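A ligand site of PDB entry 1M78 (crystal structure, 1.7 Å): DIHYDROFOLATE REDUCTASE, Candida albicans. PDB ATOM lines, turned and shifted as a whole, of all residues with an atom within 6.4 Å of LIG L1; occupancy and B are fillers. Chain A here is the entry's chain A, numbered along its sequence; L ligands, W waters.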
ATOM      1  N   ILE A   9      11.370   5.374  21.780  1.00  0.00           N
ATOM      2  CA  ILE A   9      12.064   4.002  21.505  1.00  0.00           C
ATOM      3  C   ILE A   9      12.182   3.401  22.876  1.00  0.00           C
ATOM      4  O   ILE A   9      12.756   4.008  23.812  1.00  0.00           O
ATOM      5  CB  ILE A   9      13.370   4.206  20.731  1.00  0.00           C
ATOM      6  CG1 ILE A   9      14.058   2.786  20.547  1.00  0.00           C
ATOM      7  CG2 ILE A   9      14.431   5.206  21.348  1.00  0.00           C
ATOM      8  CD1 ILE A   9      15.085   2.799  19.347  1.00  0.00           C
ATOM      9  N   VAL A  10      11.715   2.129  23.045  1.00  0.00           N
ATOM     10  CA  VAL A  10      11.767   1.455  24.340  1.00  0.00           C
ATOM     11  C   VAL A  10      11.778  -0.100  24.129  1.00  0.00           C
ATOM     12  O   VAL A  10      11.315  -0.490  23.062  1.00  0.00           O
ATOM     13  CB  VAL A  10      10.506   1.839  25.162  1.00  0.00           C
ATOM     14  CG1 VAL A  10       9.204   1.561  24.397  1.00  0.00           C
ATOM     15  CG2 VAL A  10      10.422   1.255  26.571  1.00  0.00           C
ATOM     16  N   ALA A  11      12.288  -0.768  25.118  1.00  0.00           N
ATOM     17  CA  ALA A  11      12.253  -2.275  25.111  1.00  0.00           C
ATOM     18  C   ALA A  11      11.334  -2.690  26.275  1.00  0.00           C
ATOM     19  O   ALA A  11      11.588  -2.264  27.410  1.00  0.00           O
ATOM     20  CB  ALA A  11      13.677  -2.779  25.323  1.00  0.00           C
ATOM     21  N   MET A  25      17.586  -1.849  33.953  1.00  0.00           N
ATOM     22  CA  MET A  25      16.839  -2.723  33.005  1.00  0.00           C
ATOM     23  C   MET A  25      16.983  -4.149  33.588  1.00  0.00           C
ATOM     24  O   MET A  25      18.030  -4.516  34.123  1.00  0.00           O
ATOM     25  CB  MET A  25      17.286  -2.617  31.568  1.00  0.00           C
ATOM     26  CG  MET A  25      17.061  -1.235  31.031  1.00  0.00           C
ATOM     27  SD  MET A  25      17.767  -1.089  29.365  1.00  0.00           S
ATOM     28  CE  MET A  25      16.525  -1.992  28.400  1.00  0.00           C
ATOM     29  N   GLU A  32      20.130  -6.064  21.185  1.00  0.00           N
ATOM     30  CA  GLU A  32      19.111  -4.950  21.352  1.00  0.00           C
ATOM     31  C   GLU A  32      19.815  -3.653  21.622  1.00  0.00           C
ATOM     32  O   GLU A  32      19.380  -2.656  20.994  1.00  0.00           O
ATOM     33  CB  GLU A  32      18.148  -5.281  22.504  1.00  0.00           C
ATOM     34  CG  GLU A  32      16.683  -4.813  22.381  1.00  0.00           C
ATOM     35  CD  GLU A  32      16.529  -3.306  22.592  1.00  0.00           C
ATOM     36  OE1 GLU A  32      17.263  -2.766  23.388  1.00  0.00           O
ATOM     37  OE2 GLU A  32      15.659  -2.804  21.858  1.00  0.00           O
ATOM     38  N   ILE A  33      20.805  -3.600  22.488  1.00  0.00           N
ATOM     39  CA  ILE A  33      21.592  -2.404  22.790  1.00  0.00           C
ATOM     40  C   ILE A  33      22.221  -1.874  21.487  1.00  0.00           C
ATOM     41  O   ILE A  33      22.241  -0.716  21.226  1.00  0.00           O
ATOM     42  CB  ILE A  33      22.698  -2.710  23.881  1.00  0.00           C
ATOM     43  CG1 ILE A  33      22.109  -3.284  25.137  1.00  0.00           C
ATOM     44  CG2 ILE A  33      23.678  -1.533  24.069  1.00  0.00           C
ATOM     45  CD1 ILE A  33      21.186  -2.569  26.075  1.00  0.00           C
ATOM     46  N   TYR A  35      21.094  -2.356  18.335  1.00  0.00           N
ATOM     47  CA  TYR A  35      20.009  -1.823  17.526  1.00  0.00           C
ATOM     48  C   TYR A  35      19.694  -0.362  18.036  1.00  0.00           C
ATOM     49  O   TYR A  35      19.568   0.522  17.194  1.00  0.00           O
ATOM     50  CB  TYR A  35      18.754  -2.685  17.722  1.00  0.00           C
ATOM     51  CG  TYR A  35      17.467  -2.149  17.174  1.00  0.00           C
ATOM     52  CD1 TYR A  35      16.486  -1.551  18.015  1.00  0.00           C
ATOM     53  CD2 TYR A  35      17.192  -2.235  15.815  1.00  0.00           C
ATOM     54  CE1 TYR A  35      15.292  -1.060  17.467  1.00  0.00           C
ATOM     55  CE2 TYR A  35      16.003  -1.785  15.282  1.00  0.00           C
ATOM     56  CZ  TYR A  35      15.065  -1.186  16.106  1.00  0.00           C
ATOM     57  OH  TYR A  35      13.881  -0.795  15.480  1.00  0.00           O
ATOM     58  N   PHE A  36      19.530  -0.304  19.327  1.00  0.00           N
ATOM     59  CA  PHE A  36      19.255   1.105  19.952  1.00  0.00           C
ATOM     60  C   PHE A  36      20.279   2.079  19.454  1.00  0.00           C
ATOM     61  O   PHE A  36      19.950   3.231  19.009  1.00  0.00           O
ATOM     62  CB  PHE A  36      19.141   0.942  21.470  1.00  0.00           C
ATOM     63  CG  PHE A  36      19.129   2.305  22.191  1.00  0.00           C
ATOM     64  CD1 PHE A  36      20.325   2.694  22.810  1.00  0.00           C
ATOM     65  CD2 PHE A  36      18.026   3.131  22.126  1.00  0.00           C
ATOM     66  CE1 PHE A  36      20.390   3.949  23.452  1.00  0.00           C
ATOM     67  CE2 PHE A  36      18.088   4.394  22.771  1.00  0.00           C
ATOM     68  CZ  PHE A  36      19.250   4.761  23.408  1.00  0.00           C
ATOM     69  N   THR A  58      17.343   8.906  34.240  1.00  0.00           N
ATOM     70  CA  THR A  58      18.006   8.149  33.169  1.00  0.00           C
ATOM     71  C   THR A  58      19.407   8.647  32.915  1.00  0.00           C
ATOM     72  O   THR A  58      20.352   7.846  32.871  1.00  0.00           O
ATOM     73  CB  THR A  58      17.119   7.943  31.902  1.00  0.00           C
ATOM     74  OG1 THR A  58      15.974   7.134  32.424  1.00  0.00           O
ATOM     75  CG2 THR A  58      17.845   7.081  30.832  1.00  0.00           C
ATOM     76  N   LEU A  69      25.807  10.521  25.459  1.00  0.00           N
ATOM     77  CA  LEU A  69      25.912   9.379  24.414  1.00  0.00           C
ATOM     78  C   LEU A  69      26.524  10.031  23.188  1.00  0.00           C
ATOM     79  O   LEU A  69      26.062  11.063  22.634  1.00  0.00           O
ATOM     80  CB  LEU A  69      24.523   8.875  24.279  1.00  0.00           C
ATOM     81  CG  LEU A  69      23.787   8.293  25.476  1.00  0.00           C
ATOM     82  CD1 LEU A  69      22.375   7.953  24.964  1.00  0.00           C
ATOM     83  CD2 LEU A  69      24.486   7.072  26.034  1.00  0.00           C
ATOM     84  N   ILE A 111      12.759   9.950  22.088  1.00  0.00           N
ATOM     85  CA  ILE A 111      12.601   9.927  23.573  1.00  0.00           C
ATOM     86  C   ILE A 111      13.142   8.513  24.005  1.00  0.00           C
ATOM     87  O   ILE A 111      12.568   7.525  23.554  1.00  0.00           O
ATOM     88  CB  ILE A 111      11.122  10.098  23.995  1.00  0.00           C
ATOM     89  CG1 ILE A 111      10.700  11.615  23.623  1.00  0.00           C
ATOM     90  CG2 ILE A 111      10.885   9.867  25.501  1.00  0.00           C
ATOM     91  CD1 ILE A 111       9.130  11.718  23.600  1.00  0.00           C
ATOM     92  N   ILE A 112      14.176   8.567  24.833  1.00  0.00           N
ATOM     93  CA  ILE A 112      14.815   7.316  25.256  1.00  0.00           C
ATOM     94  C   ILE A 112      14.529   6.809  26.628  1.00  0.00           C
ATOM     95  O   ILE A 112      15.141   5.788  27.044  1.00  0.00           O
ATOM     96  CB  ILE A 112      16.339   7.302  24.818  1.00  0.00           C
ATOM     97  CG1 ILE A 112      17.170   8.209  25.769  1.00  0.00           C
ATOM     98  CG2 ILE A 112      16.466   7.619  23.310  1.00  0.00           C
ATOM     99  CD1 ILE A 112      18.702   8.035  25.811  1.00  0.00           C
ATOM    100  N   GLY A 113      13.683   7.477  27.413  1.00  0.00           N
ATOM    101  CA  GLY A 113      13.301   6.998  28.746  1.00  0.00           C
ATOM    102  C   GLY A 113      13.504   8.127  29.785  1.00  0.00           C
ATOM    103  O   GLY A 113      13.974   9.185  29.425  1.00  0.00           O
ATOM    104  N   TYR A 118       8.337   8.510  29.639  1.00  0.00           N
ATOM    105  CA  TYR A 118       7.477   7.756  28.715  1.00  0.00           C
ATOM    106  C   TYR A 118       5.974   7.919  28.961  1.00  0.00           C
ATOM    107  O   TYR A 118       5.220   8.144  27.993  1.00  0.00           O
ATOM    108  CB  TYR A 118       7.822   6.241  28.726  1.00  0.00           C
ATOM    109  CG  TYR A 118       9.123   5.768  28.167  1.00  0.00           C
ATOM    110  CD1 TYR A 118       9.608   6.170  26.907  1.00  0.00           C
ATOM    111  CD2 TYR A 118       9.819   4.707  28.806  1.00  0.00           C
ATOM    112  CE1 TYR A 118      10.800   5.699  26.398  1.00  0.00           C
ATOM    113  CE2 TYR A 118      10.999   4.212  28.288  1.00  0.00           C
ATOM    114  CZ  TYR A 118      11.465   4.661  27.062  1.00  0.00           C
ATOM    115  OH  TYR A 118      12.583   4.106  26.539  1.00  0.00           O
ATOM    116  N   LEU A 131       8.675   2.989  18.652  1.00  0.00           N
ATOM    117  CA  LEU A 131       9.574   1.837  18.244  1.00  0.00           C
ATOM    118  C   LEU A 131       9.702   1.029  19.536  1.00  0.00           C
ATOM    119  O   LEU A 131      10.429   1.414  20.474  1.00  0.00           O
ATOM    120  CB  LEU A 131      10.886   2.390  17.708  1.00  0.00           C
ATOM    121  CG  LEU A 131      10.944   3.087  16.385  1.00  0.00           C
ATOM    122  CD1 LEU A 131      12.274   3.840  16.230  1.00  0.00           C
ATOM    123  CD2 LEU A 131      10.806   2.100  15.233  1.00  0.00           C
ATOM    124  N   ILE A 132       8.987  -0.071  19.584  1.00  0.00           N
ATOM    125  CA  ILE A 132       8.882  -0.935  20.699  1.00  0.00           C
ATOM    126  C   ILE A 132       9.538  -2.318  20.413  1.00  0.00           C
ATOM    127  O   ILE A 132       9.027  -2.977  19.490  1.00  0.00           O
ATOM    128  CB  ILE A 132       7.425  -1.122  21.238  1.00  0.00           C
ATOM    129  CG1 ILE A 132       6.749   0.256  21.568  1.00  0.00           C
ATOM    130  CG2 ILE A 132       7.309  -2.022  22.515  1.00  0.00           C
ATOM    131  CD1 ILE A 132       5.172   0.053  21.579  1.00  0.00           C
ATOM    132  N   THR A 133      10.503  -2.551  21.260  1.00  0.00           N
ATOM    133  CA  THR A 133      11.115  -3.974  21.139  1.00  0.00           C
ATOM    134  C   THR A 133      10.219  -4.809  22.042  1.00  0.00           C
ATOM    135  O   THR A 133      10.142  -4.559  23.282  1.00  0.00           O
ATOM    136  CB  THR A 133      12.604  -3.956  21.599  1.00  0.00           C
ATOM    137  OG1 THR A 133      13.363  -3.049  20.726  1.00  0.00           O
ATOM    138  CG2 THR A 133      13.184  -5.428  21.430  1.00  0.00           C
ATOM    139  N   TYR A 186      11.477  -6.419  16.869  1.00  0.00           N
ATOM    140  CA  TYR A 186      11.368  -4.921  16.750  1.00  0.00           C
ATOM    141  C   TYR A 186      10.024  -4.642  16.122  1.00  0.00           C
ATOM    142  O   TYR A 186       9.585  -5.264  15.182  1.00  0.00           O
ATOM    143  CB  TYR A 186      12.547  -4.420  15.893  1.00  0.00           C
ATOM    144  CG  TYR A 186      13.897  -4.819  16.457  1.00  0.00           C
ATOM    145  CD1 TYR A 186      14.239  -4.466  17.790  1.00  0.00           C
ATOM    146  CD2 TYR A 186      14.830  -5.543  15.690  1.00  0.00           C
ATOM    147  CE1 TYR A 186      15.447  -4.909  18.301  1.00  0.00           C
ATOM    148  CE2 TYR A 186      16.069  -5.902  16.201  1.00  0.00           C
ATOM    149  CZ  TYR A 186      16.356  -5.600  17.519  1.00  0.00           C
ATOM    150  OH  TYR A 186      17.573  -5.905  18.045  1.00  0.00           O
HETATM  151  C1  LIG L   1      15.889   2.353  24.751  1.00  0.00           C
HETATM  152  N1  LIG L   1      15.142   1.692  23.850  1.00  0.00           N
HETATM  153  C2  LIG L   1      15.544   0.442  23.373  1.00  0.00           C
HETATM  154  N2  LIG L   1      16.651  -0.209  23.908  1.00  0.00           N
HETATM  155  N3  LIG L   1      15.416   3.596  25.136  1.00  0.00           N
HETATM  156  N4  LIG L   1      14.779  -0.233  22.535  1.00  0.00           N
HETATM  157  C3  LIG L   1      19.201   1.728  26.667  1.00  0.00           C
HETATM  158  C4  LIG L   1      18.045   2.365  26.166  1.00  0.00           C
HETATM  159  C5  LIG L   1      17.141   1.769  25.294  1.00  0.00           C
HETATM  160  C6  LIG L   1      17.470   0.436  24.803  1.00  0.00           C
HETATM  161  C7  LIG L   1      18.658  -0.172  25.269  1.00  0.00           C
HETATM  162  C8  LIG L   1      19.494   0.403  26.152  1.00  0.00           C
HETATM  163  N5  LIG L   1      20.082   2.300  27.521  1.00  0.00           N
HETATM  164 CL1  LIG L   1      17.838   3.979  26.793  1.00  0.00          CL
HETATM  165  P1  LG2 L   2      13.211   9.143  34.243  1.00  0.00           P
HETATM  166  O1  LG2 L   2      14.443   8.940  33.437  1.00  0.00           O
HETATM  167  O2  LG2 L   2      11.942   9.158  33.512  1.00  0.00           O
HETATM  168  O3  LG2 L   2      13.471  10.577  35.021  1.00  0.00           O
HETATM  169  C1  LG2 L   2      12.348  11.101  35.795  1.00  0.00           C
HETATM  170  C2  LG2 L   2      12.722  12.610  35.985  1.00  0.00           C
HETATM  171  O4  LG2 L   2      12.595  13.305  34.754  1.00  0.00           O
HETATM  172  C3  LG2 L   2      11.774  13.333  36.984  1.00  0.00           C
HETATM  173  O5  LG2 L   2      12.311  13.088  38.294  1.00  0.00           O
HETATM  174  C4  LG2 L   2      12.022  14.822  36.480  1.00  0.00           C
HETATM  175  O6  LG2 L   2      13.295  15.362  36.834  1.00  0.00           O
HETATM  176  C5  LG2 L   2      12.117  14.598  34.985  1.00  0.00           C
HETATM  177  N1  LG2 L   2      10.850  14.686  34.351  1.00  0.00           N
HETATM  178  C6  LG2 L   2       9.908  13.699  34.338  1.00  0.00           C
HETATM  179  N2  LG2 L   2       8.840  14.046  33.633  1.00  0.00           N
HETATM  180  C7  LG2 L   2       9.155  15.336  33.253  1.00  0.00           C
HETATM  181  C8  LG2 L   2       8.383  16.241  32.481  1.00  0.00           C
HETATM  182  N3  LG2 L   2       7.186  15.868  32.045  1.00  0.00           N
HETATM  183  N4  LG2 L   2       8.968  17.437  32.252  1.00  0.00           N
HETATM  184  C9  LG2 L   2      10.189  17.716  32.776  1.00  0.00           C
HETATM  185  N5  LG2 L   2      10.981  16.952  33.496  1.00  0.00           N
HETATM  186  C10 LG2 L   2      10.345  15.754  33.688  1.00  0.00           C
HETATM  187  O7  LG2 L   2      13.131   8.135  35.381  1.00  0.00           O
HETATM  188  P2  LG2 L   2      12.271   6.982  36.042  1.00  0.00           P
HETATM  189  O8  LG2 L   2      12.756   6.572  37.355  1.00  0.00           O
HETATM  190  O9  LG2 L   2      10.821   7.165  36.003  1.00  0.00           O
HETATM  191  O10 LG2 L   2      12.625   5.728  34.999  1.00  0.00           O
HETATM  192  C11 LG2 L   2      13.840   4.984  35.281  1.00  0.00           C
HETATM  193  C12 LG2 L   2      13.533   3.534  34.932  1.00  0.00           C
HETATM  194  O11 LG2 L   2      13.271   3.473  33.482  1.00  0.00           O
HETATM  195  C13 LG2 L   2      14.598   2.490  35.216  1.00  0.00           C
HETATM  196  O12 LG2 L   2      13.981   1.278  35.718  1.00  0.00           O
HETATM  197  C14 LG2 L   2      15.195   2.271  33.815  1.00  0.00           C
HETATM  198  O13 LG2 L   2      15.792   0.965  33.758  1.00  0.00           O
HETATM  199  C15 LG2 L   2      13.968   2.379  32.931  1.00  0.00           C
HETATM  200  N6  LG2 L   2      14.264   2.622  31.476  1.00  0.00           N
HETATM  201  C16 LG2 L   2      13.919   1.513  30.664  1.00  0.00           C
HETATM  202  C17 LG2 L   2      14.235   1.618  29.312  1.00  0.00           C
HETATM  203  C18 LG2 L   2      13.788   0.393  28.410  1.00  0.00           C
HETATM  204  O14 LG2 L   2      13.910   0.514  27.203  1.00  0.00           O
HETATM  205  N7  LG2 L   2      13.257  -0.694  29.019  1.00  0.00           N
HETATM  206  C19 LG2 L   2      14.844   2.726  28.679  1.00  0.00           C
HETATM  207  C20 LG2 L   2      15.181   3.764  29.626  1.00  0.00           C
HETATM  208  C21 LG2 L   2      14.959   3.696  30.959  1.00  0.00           C
HETATM  209  P3  LG2 L   2      13.321  16.286  38.261  1.00  0.00           P
HETATM  210  O15 LG2 L   2      14.772  16.755  38.207  1.00  0.00           O
HETATM  211  O16 LG2 L   2      12.248  17.240  37.984  1.00  0.00           O
HETATM  212  O17 LG2 L   2      13.020  15.273  39.275  1.00  0.00           O
HETATM  213  O   HOH W   1      12.673  -0.453  19.891  1.00  0.00           O
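N2 of LIG L1 lies within hydrogen-bond range of OE1 of Glu 32 (2.7 Å). The backbone carbonyl oxygen of Ile 112 sits at hydrogen-bond distance from a nitrogen (N3) of LIG L1, at 2.9 Å. O of Ile 9 lies within hydrogen-bond range of N3 of LIG L1 (3.0 Å). The side-chain hydroxyl of Tyr 118 sits at hydrogen-bond distance from a nitrogen (N3) of LIG L1. The backbone NH of Ala 11 lies within hydrogen-bond range of an oxygen (O14) of LG2 L2. The backbone carbonyl oxygen (O) of Ala 11 is in hydrogen-bond range of a nitrogen (N7) of LG2 L2 (2.8 Å). The backbone NH (N) of Met 25 is in hydrogen-bond range of an oxygen (O13) of LG2 L2, at 3.3 Å. O1 of LG2 L2 sits at hydrogen-bond distance from N of Thr 58 (3.0 Å). The side-chain hydroxyl (OG1) of Thr 58 is in hydrogen-bond range of an oxygen (O1) of LG2 L2 (2.6 Å).
The side-chain hydroxyl (OG1) of Thr 133 lies within hydrogen-bond range of the side-chain carboxylate (OE2) of Glu 32 (2.6 Å). The side-chain hydroxyl (OH) of Tyr 118 is in hydrogen-bond range of the backbone carbonyl oxygen (O) of Ile 112, 3.1 Å away. The backbone carbonyl oxygen of Ile 9 lies within hydrogen-bond range of the side-chain hydroxyl of Tyr 118 (2.7 Å). N of Ile 9 is in hydrogen-bond range of O of Ile 111 (3.0 Å). The backbone carbonyl oxygen (O) of Val 10 lies within hydrogen-bond range of the backbone NH (N) of Thr 133 (2.9 Å). N of Val 10 sits at hydrogen-bond distance from O of Leu 131 (3.0 Å).
Residues that only touch LIG L1: Val 10 (3.4 Å), Ile 33 (3.4 Å), Phe 36 (3.5 Å), Ala 11 (3.6 Å), Thr 133 (3.6 Å) and Met 25 (3.9 Å). Hydrophobic or aromatic side chains within 4 Å of LIG L1: Ile 9, Ala 11, Met 25, Ile 33, Phe 36 and Ile 112.
Water W1 lies within hydrogen-bond range of OG1 of Thr 133 (2.8 Å), O of Leu 131 (3.0 Å), N4 of LIG L1 (3.4 Å) and O of Val 10 (3.4 Å).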
